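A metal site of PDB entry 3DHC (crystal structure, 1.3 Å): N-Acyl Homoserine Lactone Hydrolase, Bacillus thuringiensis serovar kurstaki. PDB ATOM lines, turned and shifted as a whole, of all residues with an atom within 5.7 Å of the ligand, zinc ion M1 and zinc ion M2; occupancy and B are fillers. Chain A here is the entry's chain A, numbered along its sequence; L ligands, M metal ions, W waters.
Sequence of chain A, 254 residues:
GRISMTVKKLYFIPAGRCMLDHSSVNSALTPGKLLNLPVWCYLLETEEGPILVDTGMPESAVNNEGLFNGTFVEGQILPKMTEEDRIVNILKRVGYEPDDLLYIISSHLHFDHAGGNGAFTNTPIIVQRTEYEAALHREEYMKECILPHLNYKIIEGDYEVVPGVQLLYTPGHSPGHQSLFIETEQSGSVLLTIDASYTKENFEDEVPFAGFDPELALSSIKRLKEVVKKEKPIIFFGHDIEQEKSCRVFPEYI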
ATOM      1  N   CYS A  18     -28.154  25.461  34.617  1.00  0.00           N
ATOM      2  CA  CYS A  18     -27.694  24.082  34.786  1.00  0.00           C
ATOM      3  C   CYS A  18     -26.993  23.950  36.115  1.00  0.00           C
ATOM      4  O   CYS A  18     -26.138  24.774  36.441  1.00  0.00           O
ATOM      5  CB  CYS A  18     -26.777  23.727  33.610  1.00  0.00           C
ATOM      6  SG  CYS A  18     -26.393  21.953  33.574  1.00  0.00           S
ATOM      7  N   MET A  19     -27.328  22.899  36.872  1.00  0.00           N
ATOM      8  CA  MET A  19     -26.552  22.610  38.116  1.00  0.00           C
ATOM      9  C   MET A  19     -25.316  21.851  37.740  1.00  0.00           C
ATOM     10  O   MET A  19     -25.364  20.882  36.948  1.00  0.00           O
ATOM     11  CB  MET A  19     -27.384  21.754  39.044  1.00  0.00           C
ATOM     12  CG  MET A  19     -28.746  22.351  39.148  1.00  0.00           C
ATOM     13  SD  MET A  19     -29.355  22.228  40.778  1.00  0.00           S
ATOM     14  CE  MET A  19     -28.007  22.882  41.789  1.00  0.00           C
ATOM     15  N   LEU A  20     -24.201  22.291  38.311  1.00  0.00           N
ATOM     16  CA  LEU A  20     -22.935  21.633  38.091  1.00  0.00           C
ATOM     17  C   LEU A  20     -22.244  21.509  39.441  1.00  0.00           C
ATOM     18  O   LEU A  20     -22.302  22.408  40.214  1.00  0.00           O
ATOM     19  CB  LEU A  20     -22.124  22.482  37.094  1.00  0.00           C
ATOM     20  CG  LEU A  20     -20.750  22.013  36.650  1.00  0.00           C
ATOM     21  CD1 LEU A  20     -20.930  20.687  35.862  1.00  0.00           C
ATOM     22  CD2 LEU A  20     -20.051  23.053  35.799  1.00  0.00           C
ATOM     23  N   LEU A  37     -25.805  27.349  37.652  1.00  0.00           N
ATOM     24  CA  LEU A  37     -25.043  28.241  36.787  1.00  0.00           C
ATOM     25  C   LEU A  37     -25.898  28.687  35.607  1.00  0.00           C
ATOM     26  O   LEU A  37     -26.801  27.963  35.137  1.00  0.00           O
ATOM     27  CB  LEU A  37     -23.850  27.455  36.181  1.00  0.00           C
ATOM     28  CG  LEU A  37     -22.825  26.952  37.192  1.00  0.00           C
ATOM     29  CD1 LEU A  37     -21.731  26.139  36.527  1.00  0.00           C
ATOM     30  CD2 LEU A  37     -22.274  28.113  37.981  1.00  0.00           C
ATOM     31  N   PRO A  38     -25.596  29.887  35.073  1.00  0.00           N
ATOM     32  CA  PRO A  38     -26.386  30.403  33.929  1.00  0.00           C
ATOM     33  C   PRO A  38     -25.992  29.731  32.655  1.00  0.00           C
ATOM     34  O   PRO A  38     -24.782  29.420  32.473  1.00  0.00           O
ATOM     35  CB  PRO A  38     -26.011  31.880  33.890  1.00  0.00           C
ATOM     36  CG  PRO A  38     -24.578  31.899  34.463  1.00  0.00           C
ATOM     37  CD  PRO A  38     -24.558  30.833  35.536  1.00  0.00           C
ATOM     38  N   VAL A  39     -26.959  29.498  31.766  1.00  0.00           N
ATOM     39  CA  VAL A  39     -26.659  29.117  30.379  1.00  0.00           C
ATOM     40  C   VAL A  39     -27.010  30.319  29.506  1.00  0.00           C
ATOM     41  O   VAL A  39     -28.090  30.937  29.684  1.00  0.00           O
ATOM     42  CB  VAL A  39     -27.496  27.885  29.960  1.00  0.00           C
ATOM     43  CG1 VAL A  39     -27.362  27.572  28.440  1.00  0.00           C
ATOM     44  CG2 VAL A  39     -27.107  26.663  30.806  1.00  0.00           C
ATOM     45  N   ILE A  77     -24.435  16.843  36.712  1.00  0.00           N
ATOM     46  CA  ILE A  77     -24.982  17.861  35.783  1.00  0.00           C
ATOM     47  C   ILE A  77     -26.500  17.675  35.769  1.00  0.00           C
ATOM     48  O   ILE A  77     -26.978  16.580  35.454  1.00  0.00           O
ATOM     49  CB  ILE A  77     -24.417  17.636  34.344  1.00  0.00           C
ATOM     50  CG1 ILE A  77     -22.871  17.745  34.388  1.00  0.00           C
ATOM     51  CG2 ILE A  77     -25.101  18.672  33.437  1.00  0.00           C
ATOM     52  CD1 ILE A  77     -22.117  17.661  33.044  1.00  0.00           C
ATOM     53  N   HIS A 108     -19.088  25.553  20.776  1.00  0.00           N
ATOM     54  CA  HIS A 108     -18.687  24.169  20.857  1.00  0.00           C
ATOM     55  C   HIS A 108     -20.008  23.347  20.935  1.00  0.00           C
ATOM     56  O   HIS A 108     -21.094  23.972  20.922  1.00  0.00           O
ATOM     57  CB  HIS A 108     -17.714  23.844  22.005  1.00  0.00           C
ATOM     58  CG  HIS A 108     -18.233  24.109  23.372  1.00  0.00           C
ATOM     59  ND1 HIS A 108     -18.793  25.307  23.774  1.00  0.00           N
ATOM     60  CD2 HIS A 108     -18.123  23.344  24.504  1.00  0.00           C
ATOM     61  CE1 HIS A 108     -18.988  25.272  25.099  1.00  0.00           C
ATOM     62  NE2 HIS A 108     -18.616  24.092  25.556  1.00  0.00           N
ATOM     63  N   HIS A 110     -21.017  21.028  23.254  1.00  0.00           N
ATOM     64  CA  HIS A 110     -21.583  20.575  24.528  1.00  0.00           C
ATOM     65  C   HIS A 110     -23.079  20.875  24.585  1.00  0.00           C
ATOM     66  O   HIS A 110     -23.584  21.795  23.939  1.00  0.00           O
ATOM     67  CB  HIS A 110     -20.833  21.185  25.667  1.00  0.00           C
ATOM     68  CG  HIS A 110     -19.450  20.602  25.820  1.00  0.00           C
ATOM     69  ND1 HIS A 110     -18.503  21.200  26.631  1.00  0.00           N
ATOM     70  CD2 HIS A 110     -18.856  19.520  25.285  1.00  0.00           C
ATOM     71  CE1 HIS A 110     -17.386  20.486  26.604  1.00  0.00           C
ATOM     72  NE2 HIS A 110     -17.554  19.455  25.795  1.00  0.00           N
ATOM     73  N   PHE A 111     -23.769  20.136  25.480  1.00  0.00           N
ATOM     74  CA  PHE A 111     -25.242  20.022  25.401  1.00  0.00           C
ATOM     75  C   PHE A 111     -25.952  21.315  25.639  1.00  0.00           C
ATOM     76  O   PHE A 111     -27.075  21.506  25.135  1.00  0.00           O
ATOM     77  CB  PHE A 111     -25.754  18.870  26.277  1.00  0.00           C
ATOM     78  CG  PHE A 111     -26.022  19.307  27.670  1.00  0.00           C
ATOM     79  CD1 PHE A 111     -27.335  19.539  28.062  1.00  0.00           C
ATOM     80  CD2 PHE A 111     -24.994  19.580  28.566  1.00  0.00           C
ATOM     81  CE1 PHE A 111     -27.638  19.997  29.321  1.00  0.00           C
ATOM     82  CE2 PHE A 111     -25.293  20.107  29.888  1.00  0.00           C
ATOM     83  CZ  PHE A 111     -26.611  20.302  30.225  1.00  0.00           C
ATOM     84  N   ASP A 112     -25.347  22.191  26.463  1.00  0.00           N
ATOM     85  CA  ASP A 112     -26.018  23.454  26.778  1.00  0.00           C
ATOM     86  C   ASP A 112     -25.611  24.582  25.872  1.00  0.00           C
ATOM     87  O   ASP A 112     -26.083  25.695  26.075  1.00  0.00           O
ATOM     88  CB  ASP A 112     -25.807  23.839  28.236  1.00  0.00           C
ATOM     89  CG  ASP A 112     -24.399  24.014  28.576  1.00  0.00           C
ATOM     90  OD1 ASP A 112     -24.015  25.085  29.154  1.00  0.00           O
ATOM     91  OD2 ASP A 112     -23.554  23.121  28.223  1.00  0.00           O
ATOM     92  N   HIS A 113     -24.813  24.255  24.839  1.00  0.00           N
ATOM     93  CA  HIS A 113     -24.457  25.247  23.817  1.00  0.00           C
ATOM     94  C   HIS A 113     -24.973  24.907  22.432  1.00  0.00           C
ATOM     95  O   HIS A 113     -25.112  25.822  21.610  1.00  0.00           O
ATOM     96  CB  HIS A 113     -22.916  25.339  23.742  1.00  0.00           C
ATOM     97  CG  HIS A 113     -22.343  25.869  24.988  1.00  0.00           C
ATOM     98  ND1 HIS A 113     -22.119  27.207  25.171  1.00  0.00           N
ATOM     99  CD2 HIS A 113     -22.032  25.262  26.144  1.00  0.00           C
ATOM    100  CE1 HIS A 113     -21.700  27.402  26.417  1.00  0.00           C
ATOM    101  NE2 HIS A 113     -21.608  26.222  27.022  1.00  0.00           N
ATOM    102  N   GLU A 140     -19.154  12.580  25.774  1.00  0.00           N
ATOM    103  CA  GLU A 140     -19.811  13.714  26.440  1.00  0.00           C
ATOM    104  C   GLU A 140     -20.718  14.473  25.474  1.00  0.00           C
ATOM    105  O   GLU A 140     -21.263  15.581  25.867  1.00  0.00           O
ATOM    106  CB  GLU A 140     -18.780  14.709  27.045  1.00  0.00           C
ATOM    107  CG  GLU A 140     -17.845  15.424  26.041  1.00  0.00           C
ATOM    108  CD  GLU A 140     -16.561  14.636  25.726  1.00  0.00           C
ATOM    109  OE1 GLU A 140     -15.598  15.264  25.251  1.00  0.00           O
ATOM    110  OE2 GLU A 140     -16.496  13.385  25.920  1.00  0.00           O
ATOM    111  N   HIS A 173     -10.932  23.204  26.582  1.00  0.00           N
ATOM    112  CA  HIS A 173     -12.150  22.782  27.300  1.00  0.00           C
ATOM    113  C   HIS A 173     -12.907  21.701  26.487  1.00  0.00           C
ATOM    114  O   HIS A 173     -13.436  20.723  27.039  1.00  0.00           O
ATOM    115  CB  HIS A 173     -13.034  24.003  27.512  1.00  0.00           C
ATOM    116  CG  HIS A 173     -14.413  23.667  27.931  1.00  0.00           C
ATOM    117  ND1 HIS A 173     -14.719  23.204  29.208  1.00  0.00           N
ATOM    118  CD2 HIS A 173     -15.588  23.694  27.245  1.00  0.00           C
ATOM    119  CE1 HIS A 173     -16.017  22.940  29.237  1.00  0.00           C
ATOM    120  NE2 HIS A 173     -16.565  23.227  28.077  1.00  0.00           N
ATOM    121  N   SER A 174     -12.947  21.894  25.160  1.00  0.00           N
ATOM    122  CA  SER A 174     -13.406  20.857  24.216  1.00  0.00           C
ATOM    123  C   SER A 174     -12.428  20.886  23.022  1.00  0.00           C
ATOM    124  O   SER A 174     -11.637  21.868  22.863  1.00  0.00           O
ATOM    125  CB  SER A 174     -14.846  21.072  23.792  1.00  0.00           C
ATOM    126  OG  SER A 174     -14.936  22.221  22.945  1.00  0.00           O
ATOM    127  N   HIS A 177     -13.200  24.074  20.743  1.00  0.00           N
ATOM    128  CA  HIS A 177     -13.842  25.233  21.380  1.00  0.00           C
ATOM    129  C   HIS A 177     -13.360  26.510  20.687  1.00  0.00           C
ATOM    130  O   HIS A 177     -12.147  26.647  20.389  1.00  0.00           O
ATOM    131  CB  HIS A 177     -13.551  25.264  22.909  1.00  0.00           C
ATOM    132  CG  HIS A 177     -14.203  26.405  23.566  1.00  0.00           C
ATOM    133  ND1 HIS A 177     -15.458  26.396  24.165  1.00  0.00           N
ATOM    134  CD2 HIS A 177     -13.772  27.696  23.619  1.00  0.00           C
ATOM    135  CE1 HIS A 177     -15.779  27.629  24.567  1.00  0.00           C
ATOM    136  NE2 HIS A 177     -14.750  28.431  24.248  1.00  0.00           N
ATOM    137  N   ILE A 194     -16.672  32.371  26.361  1.00  0.00           N
ATOM    138  CA  ILE A 194     -17.462  31.136  26.413  1.00  0.00           C
ATOM    139  C   ILE A 194     -16.735  30.202  27.372  1.00  0.00           C
ATOM    140  O   ILE A 194     -16.325  30.659  28.474  1.00  0.00           O
ATOM    141  CB  ILE A 194     -17.826  30.505  25.042  1.00  0.00           C
ATOM    142  CG1 ILE A 194     -18.076  31.586  23.956  1.00  0.00           C
ATOM    143  CG2 ILE A 194     -19.053  29.580  25.254  1.00  0.00           C
ATOM    144  CD1 ILE A 194     -19.390  32.414  24.147  1.00  0.00           C
ATOM    145  N   ASP A 195     -16.625  28.922  27.036  1.00  0.00           N
ATOM    146  CA  ASP A 195     -16.114  27.963  28.027  1.00  0.00           C
ATOM    147  C   ASP A 195     -14.595  27.845  27.990  1.00  0.00           C
ATOM    148  O   ASP A 195     -14.040  26.926  28.602  1.00  0.00           O
ATOM    149  CB  ASP A 195     -16.760  26.603  27.907  1.00  0.00           C
ATOM    150  CG  ASP A 195     -18.258  26.590  28.389  1.00  0.00           C
ATOM    151  OD1 ASP A 195     -18.770  27.659  28.745  1.00  0.00           O
ATOM    152  OD2 ASP A 195     -18.863  25.466  28.275  1.00  0.00           O
ATOM    153  N   TYR A 198     -14.894  29.191  32.567  1.00  0.00           N
ATOM    154  CA  TYR A 198     -16.225  29.291  33.139  1.00  0.00           C
ATOM    155  C   TYR A 198     -16.381  30.559  33.956  1.00  0.00           C
ATOM    156  O   TYR A 198     -17.402  31.225  33.912  1.00  0.00           O
ATOM    157  CB  TYR A 198     -16.521  28.105  34.086  1.00  0.00           C
ATOM    158  CG  TYR A 198     -16.824  26.774  33.448  1.00  0.00           C
ATOM    159  CD1 TYR A 198     -16.963  26.595  32.087  1.00  0.00           C
ATOM    160  CD2 TYR A 198     -16.964  25.671  34.237  1.00  0.00           C
ATOM    161  CE1 TYR A 198     -17.270  25.362  31.593  1.00  0.00           C
ATOM    162  CE2 TYR A 198     -17.273  24.413  33.742  1.00  0.00           C
ATOM    163  CZ  TYR A 198     -17.429  24.286  32.407  1.00  0.00           C
ATOM    164  OH  TYR A 198     -17.797  23.042  31.921  1.00  0.00           O
ATOM    165  N   ALA A 210     -13.393  22.182  34.465  1.00  0.00           N
ATOM    166  CA  ALA A 210     -13.665  21.006  33.655  1.00  0.00           C
ATOM    167  C   ALA A 210     -13.220  21.234  32.219  1.00  0.00           C
ATOM    168  O   ALA A 210     -13.503  22.289  31.601  1.00  0.00           O
ATOM    169  CB  ALA A 210     -15.153  20.712  33.664  1.00  0.00           C
ATOM    170  N   GLY A 211     -12.617  20.211  31.639  1.00  0.00           N
ATOM    171  CA  GLY A 211     -12.214  20.299  30.241  1.00  0.00           C
ATOM    172  C   GLY A 211     -11.617  19.016  29.725  1.00  0.00           C
ATOM    173  O   GLY A 211     -11.091  18.200  30.482  1.00  0.00           O
ATOM    174  N   PHE A 212     -11.697  18.849  28.407  1.00  0.00           N
ATOM    175  CA  PHE A 212     -11.143  17.698  27.739  1.00  0.00           C
ATOM    176  C   PHE A 212      -9.600  17.578  27.876  1.00  0.00           C
ATOM    177  O   PHE A 212      -9.061  16.469  28.090  1.00  0.00           O
ATOM    178  CB  PHE A 212     -11.640  17.745  26.296  1.00  0.00           C
ATOM    179  CG  PHE A 212     -10.607  17.535  25.251  1.00  0.00           C
ATOM    180  CD1 PHE A 212     -10.291  16.258  24.838  1.00  0.00           C
ATOM    181  CD2 PHE A 212     -10.050  18.643  24.563  1.00  0.00           C
ATOM    182  CE1 PHE A 212      -9.360  16.048  23.838  1.00  0.00           C
ATOM    183  CE2 PHE A 212      -9.112  18.445  23.566  1.00  0.00           C
ATOM    184  CZ  PHE A 212      -8.784  17.136  23.204  1.00  0.00           C
ATOM    185  N   GLY A 238     -17.920  32.240  30.712  1.00  0.00           N
ATOM    186  CA  GLY A 238     -19.009  31.375  30.219  1.00  0.00           C
ATOM    187  C   GLY A 238     -20.122  30.988  31.219  1.00  0.00           C
ATOM    188  O   GLY A 238     -21.284  30.852  30.804  1.00  0.00           O
ATOM    189  N   HIS A 239     -19.779  30.783  32.479  1.00  0.00           N
ATOM    190  CA  HIS A 239     -20.780  30.266  33.479  1.00  0.00           C
ATOM    191  C   HIS A 239     -20.377  30.824  34.828  1.00  0.00           C
ATOM    192  O   HIS A 239     -19.973  30.041  35.719  1.00  0.00           O
ATOM    193  CB  HIS A 239     -20.706  28.715  33.547  1.00  0.00           C
ATOM    194  CG  HIS A 239     -21.146  28.030  32.291  1.00  0.00           C
ATOM    195  ND1 HIS A 239     -22.458  28.036  31.826  1.00  0.00           N
ATOM    196  CD2 HIS A 239     -20.444  27.249  31.448  1.00  0.00           C
ATOM    197  CE1 HIS A 239     -22.514  27.325  30.717  1.00  0.00           C
ATOM    198  NE2 HIS A 239     -21.320  26.808  30.498  1.00  0.00           N
HETATM  199  C1  LIG L   1     -21.408  22.779  31.741  1.00  0.00           C
HETATM  200  C2  LIG L   1     -20.672  19.711  29.775  1.00  0.00           C
HETATM  201  C3  LIG L   1     -20.483  22.835  29.414  1.00  0.00           C
HETATM  202  O1  LIG L   1     -21.349  19.806  28.723  1.00  0.00           O
HETATM  203  N1  LIG L   1     -20.606  20.687  30.673  1.00  0.00           N
HETATM  204  C4  LIG L   1     -21.202  21.998  30.452  1.00  0.00           C
HETATM  205  O2  LIG L   1     -20.945  23.773  28.921  1.00  0.00           O
HETATM  206  O3  LIG L   1     -19.400  22.565  29.065  1.00  0.00           O
HETATM  207  C5  LIG L   1     -22.860  23.301  31.842  1.00  0.00           C
HETATM  208  S1  LIG L   1     -23.045  24.375  33.278  1.00  0.00           S
HETATM  209  C6  LIG L   1     -19.830  18.490  30.100  1.00  0.00           C
HETATM  210  C7  LIG L   1     -18.450  18.589  29.373  1.00  0.00           C
HETATM  211  C8  LIG L   1     -17.435  19.435  30.183  1.00  0.00           C
HETATM  212  C9  LIG L   1     -15.929  19.462  29.828  1.00  0.00           C
HETATM  213  C10 LIG L   1     -15.477  18.191  29.162  1.00  0.00           C
HETATM  214 ZN    ZN M   1     -20.755  25.724  28.828  1.00  0.00          ZN
HETATM  215 ZN    ZN M   2     -18.497  23.194  27.470  1.00  0.00          ZN
HETATM  216  O   HOH W   1     -22.030  18.119  26.692  1.00  0.00           O
HETATM  217  O   HOH W   2     -14.027  15.613  28.221  1.00  0.00           O
HETATM  218  O   HOH W   3     -18.622  20.488  33.222  1.00  0.00           O
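OH of Tyr 198 sits close to O3 of the ligand, at 3.3 Å.
O of Cys 18 sits at hydrogen-bond distance from N of Leu 37.
ND1 of His 239 sits at hydrogen-bond distance from O of Pro 38 (2.8 Å).
A ring nitrogen (NE2) of His 239 sits close to the side-chain carboxylate (OD1) of Asp 112 (3.5 Å).
A ring nitrogen (ND1) of His 173 is in hydrogen-bond range of the backbone carbonyl oxygen (O) of Ala 210, at 2.8 Å.
A ring nitrogen (NE2) of His 113 sits close to the side-chain carboxylate (OD1) of Asp 112, at 3.4 Å.
The backbone carbonyl oxygen (O) of His 173 lies within hydrogen-bond range of the backbone NH (N) of Phe 212.
A ring nitrogen (NE2) of His 177 sits close to the backbone NH of Asp 195, 3.4 Å away.
The backbone NH (N) of His 239 sits at hydrogen-bond distance from the backbone carbonyl oxygen (O) of Tyr 198 (2.8 Å).
An oxygen (O2) of the ligand sits close to the side-chain carboxylate (OD2) of Asp 112 (2.8 Å).
Merely in contact with the ligand: Phe 111, Cys 18, Ile 77, Gly 211, Phe 212 and Leu 37.
14 residues have an atom within 4 Å of the ligand: Cys 18, Leu 37, Ile 77, His 108, His 110, Phe 111, Asp 112, His 113, His 173, Asp 195, Tyr 198, Gly 211, Phe 212 and His 239.
Merely in contact with zinc ion M1: Asp 112.
Four residues have an atom within 4 Å of zinc ion M1: Asp 112, His 113, Asp 195 and His 239.
The nearest printed residue that does not touch zinc ion M1 is His 108 (4.2 Å).
Within 4 Å of zinc ion M2: His 108, His 110, His 173 and Asp 195.
Zinc ion M1 is bound by an oxygen (O2) of the ligand, the side-chain carboxylate (OD2) of Asp 195, a ring nitrogen (NE2) of His 113 and a ring nitrogen (NE2) of His 239.
Zinc ion M1 has four donor atoms within binding distance.
Slightly farther from zinc ion M1 lies OD1 of Asp 195 (2.8 Å).
Zinc ion M2 is bound by O3 of the ligand (1.9 Å), NE2 of His 173 (2.0 Å), NE2 of His 108 (2.1 Å), ND1 of His 110 (2.2 Å) and OD2 of Asp 195 (2.4 Å).
Water W1 lies within hydrogen-bond range of an oxygen (O1) of the ligand, the backbone carbonyl oxygen (O) of Glu 140 and the backbone NH (N) of Phe 111.
Water W3 lies within hydrogen-bond range of the side-chain hydroxyl of Tyr 198 (3.0 Å) and a nitrogen (N1) of the ligand (3.2 Å).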
